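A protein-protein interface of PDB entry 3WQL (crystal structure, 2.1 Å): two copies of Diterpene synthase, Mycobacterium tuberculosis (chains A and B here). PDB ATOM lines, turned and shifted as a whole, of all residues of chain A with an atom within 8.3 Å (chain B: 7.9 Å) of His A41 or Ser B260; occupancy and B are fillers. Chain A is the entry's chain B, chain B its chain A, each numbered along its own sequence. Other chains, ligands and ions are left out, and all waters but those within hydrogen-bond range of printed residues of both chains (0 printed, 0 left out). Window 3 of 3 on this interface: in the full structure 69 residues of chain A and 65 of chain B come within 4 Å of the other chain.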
ATOM      1  N   GLY A  35      17.213 -24.601 -14.577  1.00  0.00           N
ATOM      2  CA  GLY A  35      16.238 -25.043 -13.603  1.00  0.00           C
ATOM      3  C   GLY A  35      15.343 -23.931 -13.107  1.00  0.00           C
ATOM      4  O   GLY A  35      14.683 -24.087 -12.083  1.00  0.00           O
ATOM      5  N   THR A  36      15.311 -22.813 -13.831  1.00  0.00           N
ATOM      6  CA  THR A  36      14.494 -21.670 -13.427  1.00  0.00           C
ATOM      7  C   THR A  36      13.009 -21.996 -13.241  1.00  0.00           C
ATOM      8  O   THR A  36      12.354 -21.421 -12.374  1.00  0.00           O
ATOM      9  CB  THR A  36      14.636 -20.501 -14.432  1.00  0.00           C
ATOM     10  OG1 THR A  36      16.008 -20.094 -14.497  1.00  0.00           O
ATOM     11  CG2 THR A  36      13.797 -19.301 -13.988  1.00  0.00           C
ATOM     12  N   ARG A  37      12.477 -22.910 -14.048  1.00  0.00           N
ATOM     13  CA  ARG A  37      11.066 -23.300 -13.930  1.00  0.00           C
ATOM     14  C   ARG A  37      10.763 -23.948 -12.578  1.00  0.00           C
ATOM     15  O   ARG A  37       9.754 -23.636 -11.940  1.00  0.00           O
ATOM     16  CB  ARG A  37      10.689 -24.275 -15.045  1.00  0.00           C
ATOM     17  CG  ARG A  37      10.039 -23.625 -16.255  1.00  0.00           C
ATOM     18  CD  ARG A  37       8.528 -23.744 -16.162  1.00  0.00           C
ATOM     19  NE  ARG A  37       8.129 -25.133 -15.938  1.00  0.00           N
ATOM     20  CZ  ARG A  37       6.869 -25.549 -15.829  1.00  0.00           C
ATOM     21  NH1 ARG A  37       5.868 -24.680 -15.925  1.00  0.00           N
ATOM     22  NH2 ARG A  37       6.611 -26.836 -15.617  1.00  0.00           N
ATOM     23  N   ARG A  38      11.634 -24.862 -12.154  1.00  0.00           N
ATOM     24  CA  ARG A  38      11.468 -25.543 -10.874  1.00  0.00           C
ATOM     25  C   ARG A  38      11.624 -24.489  -9.781  1.00  0.00           C
ATOM     26  O   ARG A  38      10.819 -24.414  -8.852  1.00  0.00           O
ATOM     27  CB  ARG A  38      12.536 -26.632 -10.717  1.00  0.00           C
ATOM     28  CG  ARG A  38      12.336 -27.551  -9.523  1.00  0.00           C
ATOM     29  CD  ARG A  38      13.401 -28.652  -9.476  1.00  0.00           C
ATOM     30  NE  ARG A  38      13.437 -29.428 -10.709  1.00  0.00           N
ATOM     31  CZ  ARG A  38      14.332 -30.373 -10.983  1.00  0.00           C
ATOM     32  NH1 ARG A  38      15.279 -30.675 -10.106  1.00  0.00           N
ATOM     33  NH2 ARG A  38      14.290 -31.006 -12.147  1.00  0.00           N
ATOM     34  N   TRP A  39      12.659 -23.664  -9.912  1.00  0.00           N
ATOM     35  CA  TRP A  39      12.932 -22.595  -8.952  1.00  0.00           C
ATOM     36  C   TRP A  39      11.712 -21.688  -8.729  1.00  0.00           C
ATOM     37  O   TRP A  39      11.347 -21.379  -7.588  1.00  0.00           O
ATOM     38  CB  TRP A  39      14.105 -21.740  -9.445  1.00  0.00           C
ATOM     39  CG  TRP A  39      14.328 -20.507  -8.617  1.00  0.00           C
ATOM     40  CD1 TRP A  39      14.991 -20.430  -7.424  1.00  0.00           C
ATOM     41  CD2 TRP A  39      13.832 -19.187  -8.886  1.00  0.00           C
ATOM     42  NE1 TRP A  39      14.936 -19.149  -6.933  1.00  0.00           N
ATOM     43  CE2 TRP A  39      14.231 -18.364  -7.808  1.00  0.00           C
ATOM     44  CE3 TRP A  39      13.089 -18.619  -9.930  1.00  0.00           C
ATOM     45  CZ2 TRP A  39      13.908 -16.995  -7.743  1.00  0.00           C
ATOM     46  CZ3 TRP A  39      12.770 -17.254  -9.870  1.00  0.00           C
ATOM     47  CH2 TRP A  39      13.180 -16.463  -8.783  1.00  0.00           C
ATOM     48  N   PHE A  40      11.093 -21.255  -9.824  1.00  0.00           N
ATOM     49  CA  PHE A  40       9.933 -20.368  -9.762  1.00  0.00           C
ATOM     50  C   PHE A  40       8.783 -20.959  -8.942  1.00  0.00           C
ATOM     51  O   PHE A  40       8.186 -20.278  -8.106  1.00  0.00           O
ATOM     52  CB  PHE A  40       9.447 -20.073 -11.181  1.00  0.00           C
ATOM     53  CG  PHE A  40       8.357 -19.041 -11.254  1.00  0.00           C
ATOM     54  CD1 PHE A  40       8.585 -17.739 -10.822  1.00  0.00           C
ATOM     55  CD2 PHE A  40       7.114 -19.363 -11.799  1.00  0.00           C
ATOM     56  CE1 PHE A  40       7.592 -16.763 -10.932  1.00  0.00           C
ATOM     57  CE2 PHE A  40       6.113 -18.399 -11.916  1.00  0.00           C
ATOM     58  CZ  PHE A  40       6.354 -17.092 -11.480  1.00  0.00           C
ATOM     59  N   HIS A  41       8.482 -22.226  -9.188  1.00  0.00           N
ATOM     60  CA  HIS A  41       7.403 -22.916  -8.495  1.00  0.00           C
ATOM     61  C   HIS A  41       7.655 -23.152  -7.014  1.00  0.00           C
ATOM     62  O   HIS A  41       6.708 -23.252  -6.232  1.00  0.00           O
ATOM     63  CB  HIS A  41       7.128 -24.256  -9.182  1.00  0.00           C
ATOM     64  CG  HIS A  41       6.331 -24.131 -10.441  1.00  0.00           C
ATOM     65  ND1 HIS A  41       4.952 -24.088 -10.444  1.00  0.00           N
ATOM     66  CD2 HIS A  41       6.716 -23.976 -11.730  1.00  0.00           C
ATOM     67  CE1 HIS A  41       4.522 -23.910 -11.680  1.00  0.00           C
ATOM     68  NE2 HIS A  41       5.572 -23.838 -12.479  1.00  0.00           N
ATOM     69  N   LEU A  42       8.927 -23.235  -6.628  1.00  0.00           N
ATOM     70  CA  LEU A  42       9.292 -23.480  -5.236  1.00  0.00           C
ATOM     71  C   LEU A  42       9.570 -22.218  -4.444  1.00  0.00           C
ATOM     72  O   LEU A  42       9.178 -22.115  -3.286  1.00  0.00           O
ATOM     73  CB  LEU A  42      10.534 -24.373  -5.162  1.00  0.00           C
ATOM     74  CG  LEU A  42      10.473 -25.746  -5.831  1.00  0.00           C
ATOM     75  CD1 LEU A  42      11.847 -26.381  -5.789  1.00  0.00           C
ATOM     76  CD2 LEU A  42       9.446 -26.627  -5.140  1.00  0.00           C
ATOM     77  N   GLU A  43      10.251 -21.256  -5.061  1.00  0.00           N
ATOM     78  CA  GLU A  43      10.604 -20.035  -4.354  1.00  0.00           C
ATOM     79  C   GLU A  43       9.754 -18.814  -4.654  1.00  0.00           C
ATOM     80  O   GLU A  43       9.931 -17.773  -4.029  1.00  0.00           O
ATOM     81  CB  GLU A  43      12.079 -19.714  -4.601  1.00  0.00           C
ATOM     82  CG  GLU A  43      13.024 -20.818  -4.158  1.00  0.00           C
ATOM     83  CD  GLU A  43      12.808 -21.233  -2.710  1.00  0.00           C
ATOM     84  OE1 GLU A  43      12.661 -20.338  -1.853  1.00  0.00           O
ATOM     85  OE2 GLU A  43      12.790 -22.452  -2.426  1.00  0.00           O
ATOM     86  N   CYS A  44       8.833 -18.931  -5.602  1.00  0.00           N
ATOM     87  CA  CYS A  44       7.964 -17.810  -5.945  1.00  0.00           C
ATOM     88  C   CYS A  44       6.517 -18.250  -5.918  1.00  0.00           C
ATOM     89  O   CYS A  44       6.218 -19.425  -5.725  1.00  0.00           O
ATOM     90  CB  CYS A  44       8.272 -17.281  -7.349  1.00  0.00           C
ATOM     91  SG  CYS A  44       9.907 -16.627  -7.558  1.00  0.00           S
ATOM     92  N   ASN A  45       5.621 -17.296  -6.128  1.00  0.00           N
ATOM     93  CA  ASN A  45       4.200 -17.587  -6.161  1.00  0.00           C
ATOM     94  C   ASN A  45       3.755 -17.510  -7.618  1.00  0.00           C
ATOM     95  O   ASN A  45       3.407 -16.442  -8.113  1.00  0.00           O
ATOM     96  CB  ASN A  45       3.429 -16.565  -5.333  1.00  0.00           C
ATOM     97  CG  ASN A  45       2.029 -17.029  -5.010  1.00  0.00           C
ATOM     98  OD1 ASN A  45       1.350 -17.624  -5.854  1.00  0.00           O
ATOM     99  ND2 ASN A  45       1.582 -16.755  -3.790  1.00  0.00           N
ATOM    100  N   PRO A  46       3.775 -18.644  -8.330  1.00  0.00           N
ATOM    101  CA  PRO A  46       3.365 -18.645  -9.736  1.00  0.00           C
ATOM    102  C   PRO A  46       1.942 -18.145 -10.001  1.00  0.00           C
ATOM    103  O   PRO A  46       1.545 -17.978 -11.151  1.00  0.00           O
ATOM    104  CB  PRO A  46       3.581 -20.103 -10.162  1.00  0.00           C
ATOM    105  CG  PRO A  46       3.466 -20.870  -8.880  1.00  0.00           C
ATOM    106  CD  PRO A  46       4.199 -19.989  -7.904  1.00  0.00           C
ATOM    107  N   GLN A  47       1.175 -17.898  -8.942  1.00  0.00           N
ATOM    108  CA  GLN A  47      -0.184 -17.407  -9.126  1.00  0.00           C
ATOM    109  C   GLN A  47      -0.171 -15.925  -9.495  1.00  0.00           C
ATOM    110  O   GLN A  47      -0.898 -15.496 -10.395  1.00  0.00           O
ATOM    111  CB  GLN A  47      -1.024 -17.592  -7.853  1.00  0.00           C
ATOM    112  CG  GLN A  47      -1.273 -19.037  -7.428  1.00  0.00           C
ATOM    113  CD  GLN A  47      -2.208 -19.139  -6.220  1.00  0.00           C
ATOM    114  OE1 GLN A  47      -2.391 -20.215  -5.646  1.00  0.00           O
ATOM    115  NE2 GLN A  47      -2.805 -18.014  -5.836  1.00  0.00           N
ATOM    116  N   TYR A  51       7.158 -13.933 -13.617  1.00  0.00           N
ATOM    117  CA  TYR A  51       8.232 -14.859 -13.960  1.00  0.00           C
ATOM    118  C   TYR A  51       9.443 -14.129 -14.549  1.00  0.00           C
ATOM    119  O   TYR A  51      10.570 -14.291 -14.078  1.00  0.00           O
ATOM    120  CB  TYR A  51       7.707 -15.875 -14.974  1.00  0.00           C
ATOM    121  CG  TYR A  51       8.676 -16.970 -15.343  1.00  0.00           C
ATOM    122  CD1 TYR A  51       8.853 -18.075 -14.518  1.00  0.00           C
ATOM    123  CD2 TYR A  51       9.409 -16.906 -16.528  1.00  0.00           C
ATOM    124  CE1 TYR A  51       9.734 -19.094 -14.863  1.00  0.00           C
ATOM    125  CE2 TYR A  51      10.295 -17.919 -16.883  1.00  0.00           C
ATOM    126  CZ  TYR A  51      10.450 -19.011 -16.046  1.00  0.00           C
ATOM    127  OH  TYR A  51      11.316 -20.026 -16.393  1.00  0.00           O
ATOM    128  N   TYR A 234      19.455 -20.589  -6.815  1.00  0.00           N
ATOM    129  CA  TYR A 234      19.664 -20.813  -5.378  1.00  0.00           C
ATOM    130  C   TYR A 234      21.120 -20.462  -5.038  1.00  0.00           C
ATOM    131  O   TYR A 234      21.483 -20.302  -3.875  1.00  0.00           O
ATOM    132  CB  TYR A 234      19.413 -22.280  -5.009  1.00  0.00           C
ATOM    133  CG  TYR A 234      17.959 -22.641  -4.832  1.00  0.00           C
ATOM    134  CD1 TYR A 234      17.289 -22.356  -3.643  1.00  0.00           C
ATOM    135  CD2 TYR A 234      17.255 -23.280  -5.848  1.00  0.00           C
ATOM    136  CE1 TYR A 234      15.953 -22.707  -3.469  1.00  0.00           C
ATOM    137  CE2 TYR A 234      15.926 -23.633  -5.690  1.00  0.00           C
ATOM    138  CZ  TYR A 234      15.279 -23.349  -4.500  1.00  0.00           C
ATOM    139  OH  TYR A 234      13.971 -23.736  -4.336  1.00  0.00           O
ATOM    140  N   PRO B 257       8.711 -33.703 -15.139  1.00  0.00           N
ATOM    141  CA  PRO B 257       8.171 -33.078 -13.925  1.00  0.00           C
ATOM    142  C   PRO B 257       7.007 -32.106 -14.136  1.00  0.00           C
ATOM    143  O   PRO B 257       6.997 -31.314 -15.078  1.00  0.00           O
ATOM    144  CB  PRO B 257       9.395 -32.390 -13.329  1.00  0.00           C
ATOM    145  CG  PRO B 257      10.484 -33.342 -13.670  1.00  0.00           C
ATOM    146  CD  PRO B 257      10.185 -33.681 -15.119  1.00  0.00           C
ATOM    147  N   ASP B 258       6.026 -32.185 -13.243  1.00  0.00           N
ATOM    148  CA  ASP B 258       4.862 -31.310 -13.288  1.00  0.00           C
ATOM    149  C   ASP B 258       4.678 -30.705 -11.904  1.00  0.00           C
ATOM    150  O   ASP B 258       3.840 -31.154 -11.120  1.00  0.00           O
ATOM    151  CB  ASP B 258       3.598 -32.086 -13.677  1.00  0.00           C
ATOM    152  CG  ASP B 258       2.344 -31.215 -13.654  1.00  0.00           C
ATOM    153  OD1 ASP B 258       1.237 -31.741 -13.911  1.00  0.00           O
ATOM    154  OD2 ASP B 258       2.466 -30.002 -13.377  1.00  0.00           O
ATOM    155  N   TYR B 259       5.482 -29.692 -11.605  1.00  0.00           N
ATOM    156  CA  TYR B 259       5.406 -29.025 -10.317  1.00  0.00           C
ATOM    157  C   TYR B 259       4.030 -28.383 -10.267  1.00  0.00           C
ATOM    158  O   TYR B 259       3.392 -28.316  -9.215  1.00  0.00           O
ATOM    159  CB  TYR B 259       6.492 -27.948 -10.209  1.00  0.00           C
ATOM    160  CG  TYR B 259       7.799 -28.308 -10.889  1.00  0.00           C
ATOM    161  CD1 TYR B 259       8.016 -28.005 -12.232  1.00  0.00           C
ATOM    162  CD2 TYR B 259       8.807 -28.976 -10.197  1.00  0.00           C
ATOM    163  CE1 TYR B 259       9.204 -28.357 -12.866  1.00  0.00           C
ATOM    164  CE2 TYR B 259       9.995 -29.335 -10.823  1.00  0.00           C
ATOM    165  CZ  TYR B 259      10.189 -29.024 -12.154  1.00  0.00           C
ATOM    166  OH  TYR B 259      11.365 -29.378 -12.778  1.00  0.00           O
ATOM    167  N   SER B 260       3.585 -27.934 -11.438  1.00  0.00           N
ATOM    168  CA  SER B 260       2.296 -27.274 -11.607  1.00  0.00           C
ATOM    169  C   SER B 260       1.141 -28.072 -11.014  1.00  0.00           C
ATOM    170  O   SER B 260       0.041 -27.545 -10.839  1.00  0.00           O
ATOM    171  CB  SER B 260       2.033 -27.026 -13.098  1.00  0.00           C
ATOM    172  OG  SER B 260       3.118 -26.339 -13.706  1.00  0.00           O
ATOM    173  N   ALA B 261       1.389 -29.339 -10.700  1.00  0.00           N
ATOM    174  CA  ALA B 261       0.351 -30.190 -10.134  1.00  0.00           C
ATOM    175  C   ALA B 261       0.872 -31.105  -9.032  1.00  0.00           C
ATOM    176  O   ALA B 261       0.224 -32.090  -8.685  1.00  0.00           O
ATOM    177  CB  ALA B 261      -0.291 -31.021 -11.237  1.00  0.00           C
ATOM    178  N   MET B 262       2.042 -30.786  -8.482  1.00  0.00           N
ATOM    179  CA  MET B 262       2.614 -31.600  -7.412  1.00  0.00           C
ATOM    180  C   MET B 262       1.933 -31.317  -6.078  1.00  0.00           C
ATOM    181  O   MET B 262       1.256 -30.301  -5.916  1.00  0.00           O
ATOM    182  CB  MET B 262       4.123 -31.352  -7.286  1.00  0.00           C
ATOM    183  CG  MET B 262       4.964 -32.036  -8.363  1.00  0.00           C
ATOM    184  SD  MET B 262       6.751 -31.856  -8.121  1.00  0.00           S
ATOM    185  CE  MET B 262       7.051 -33.042  -6.825  1.00  0.00           C
ATOM    186  N   SER B 263       2.114 -32.226  -5.127  1.00  0.00           N
ATOM    187  CA  SER B 263       1.524 -32.084  -3.802  1.00  0.00           C
ATOM    188  C   SER B 263       2.255 -31.027  -2.985  1.00  0.00           C
ATOM    189  O   SER B 263       3.472 -30.875  -3.098  1.00  0.00           O
ATOM    190  CB  SER B 263       1.569 -33.419  -3.059  1.00  0.00           C
ATOM    191  OG  SER B 263       1.125 -33.270  -1.721  1.00  0.00           O
ATOM    192  N   LEU B 267       6.338 -30.306  -2.403  1.00  0.00           N
ATOM    193  CA  LEU B 267       6.975 -29.026  -2.680  1.00  0.00           C
ATOM    194  C   LEU B 267       7.853 -28.592  -1.512  1.00  0.00           C
ATOM    195  O   LEU B 267       8.939 -28.048  -1.715  1.00  0.00           O
ATOM    196  CB  LEU B 267       5.921 -27.953  -2.974  1.00  0.00           C
ATOM    197  CG  LEU B 267       5.109 -28.125  -4.264  1.00  0.00           C
ATOM    198  CD1 LEU B 267       4.139 -26.966  -4.412  1.00  0.00           C
ATOM    199  CD2 LEU B 267       6.040 -28.187  -5.468  1.00  0.00           C
ATOM    200  N   ARG B 271      11.831 -28.137  -1.650  1.00  0.00           N
ATOM    201  CA  ARG B 271      12.127 -26.835  -1.088  1.00  0.00           C
ATOM    202  C   ARG B 271      13.172 -26.919   0.030  1.00  0.00           C
ATOM    203  O   ARG B 271      14.197 -26.240  -0.018  1.00  0.00           O
ATOM    204  CB  ARG B 271      10.830 -26.226  -0.552  1.00  0.00           C
ATOM    205  CG  ARG B 271      10.808 -24.720  -0.481  1.00  0.00           C
ATOM    206  CD  ARG B 271       9.604 -24.183  -1.237  1.00  0.00           C
ATOM    207  NE  ARG B 271       8.373 -24.839  -0.817  1.00  0.00           N
ATOM    208  CZ  ARG B 271       7.174 -24.590  -1.336  1.00  0.00           C
ATOM    209  NH1 ARG B 271       7.031 -23.691  -2.298  1.00  0.00           N
ATOM    210  NH2 ARG B 271       6.113 -25.255  -0.896  1.00  0.00           N
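The side-chain hydroxyl (OH) of Tyr B259 is in hydrogen-bond range of the guanidinium group (NE) of Arg A38.
The backbone carbonyl oxygen (O) of Leu A42 lies within hydrogen-bond range of the guanidinium group (NH1) of Arg B271, at 2.8 Å.
OD2 of Asp B258 sits close to N of Ser B260, at 3.0 Å.
The side-chain hydroxyl of Tyr A234 is in hydrogen-bond range of the side-chain carboxylate of Glu A43 (2.6 Å).
The backbone carbonyl oxygen (O) of Leu B267 sits close to the guanidinium group (NE) of Arg B271 (3.4 Å).
No position is printed for both chains.
Of the 9 pairs that touch across the chains among the printed residues, none has its exchanged pair printed and touching as well.
His A41 touches just these residues of chain B: Tyr B259, Ser B260 and Arg B271.
Of chain A, only Arg A37 (3.9 Å) and His A41 (3.5 Å) come within 4 Å of Ser B260.
Printed residues of chain A within 4 Å of Leu B267: Leu A42 (3.7 Å).
Of the printed residues of chain A, Arg B271 touches His A41, Leu A42 and Glu A43.
Printed residues of chain B within 4 Å of Leu A42: Leu B267 and Arg B271.
Of the printed residues of chain A, Tyr B259 touches Arg A37, Arg A38 and His A41.
Printed residues of chain B within 4 Å of Glu A43: Arg B271.
Gly A35 touches none of the printed residues of chain B.
The nearest residue of chain B that does not touch His A41 is Leu B267 (4.9 Å).
The nearest residue of chain A that does not touch Ser B260 is Pro A46 (7.1 Å).
Arg A37 touches Tyr B259 (NH2 to CD1, 3.8 Å).
OG of Ser B260 touches NH1 of Arg A37, 3.9 Å away.
CG of His A41 touches CB of Tyr B259, at 3.8 Å.
OG of Ser B260 touches CE1 of His A41 (3.5 Å).
NH1 of Arg B271 touches O of His A41, 3.97 Å away.
CD2 of Leu A42 touches O of Leu B267, 3.7 Å away.
OE2 of Glu A43 touches CG of Arg B271, at 3.6 Å.
Of the 15 printed residues of chain A, 5 touch a printed residue of chain B.
Of the 9 printed residues of chain B, 4 touch a printed residue of chain A.
Printed residues of chain B that touch a printed residue of chain A: Tyr B259, Ser B260, Leu B267 and Arg B271.
Hydrophobic or aromatic side chains of chain B within 4 Å of the printed part of chain A: Tyr B259 and Leu B267.
Among the printed residues, 9 pairs touch across the chains.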
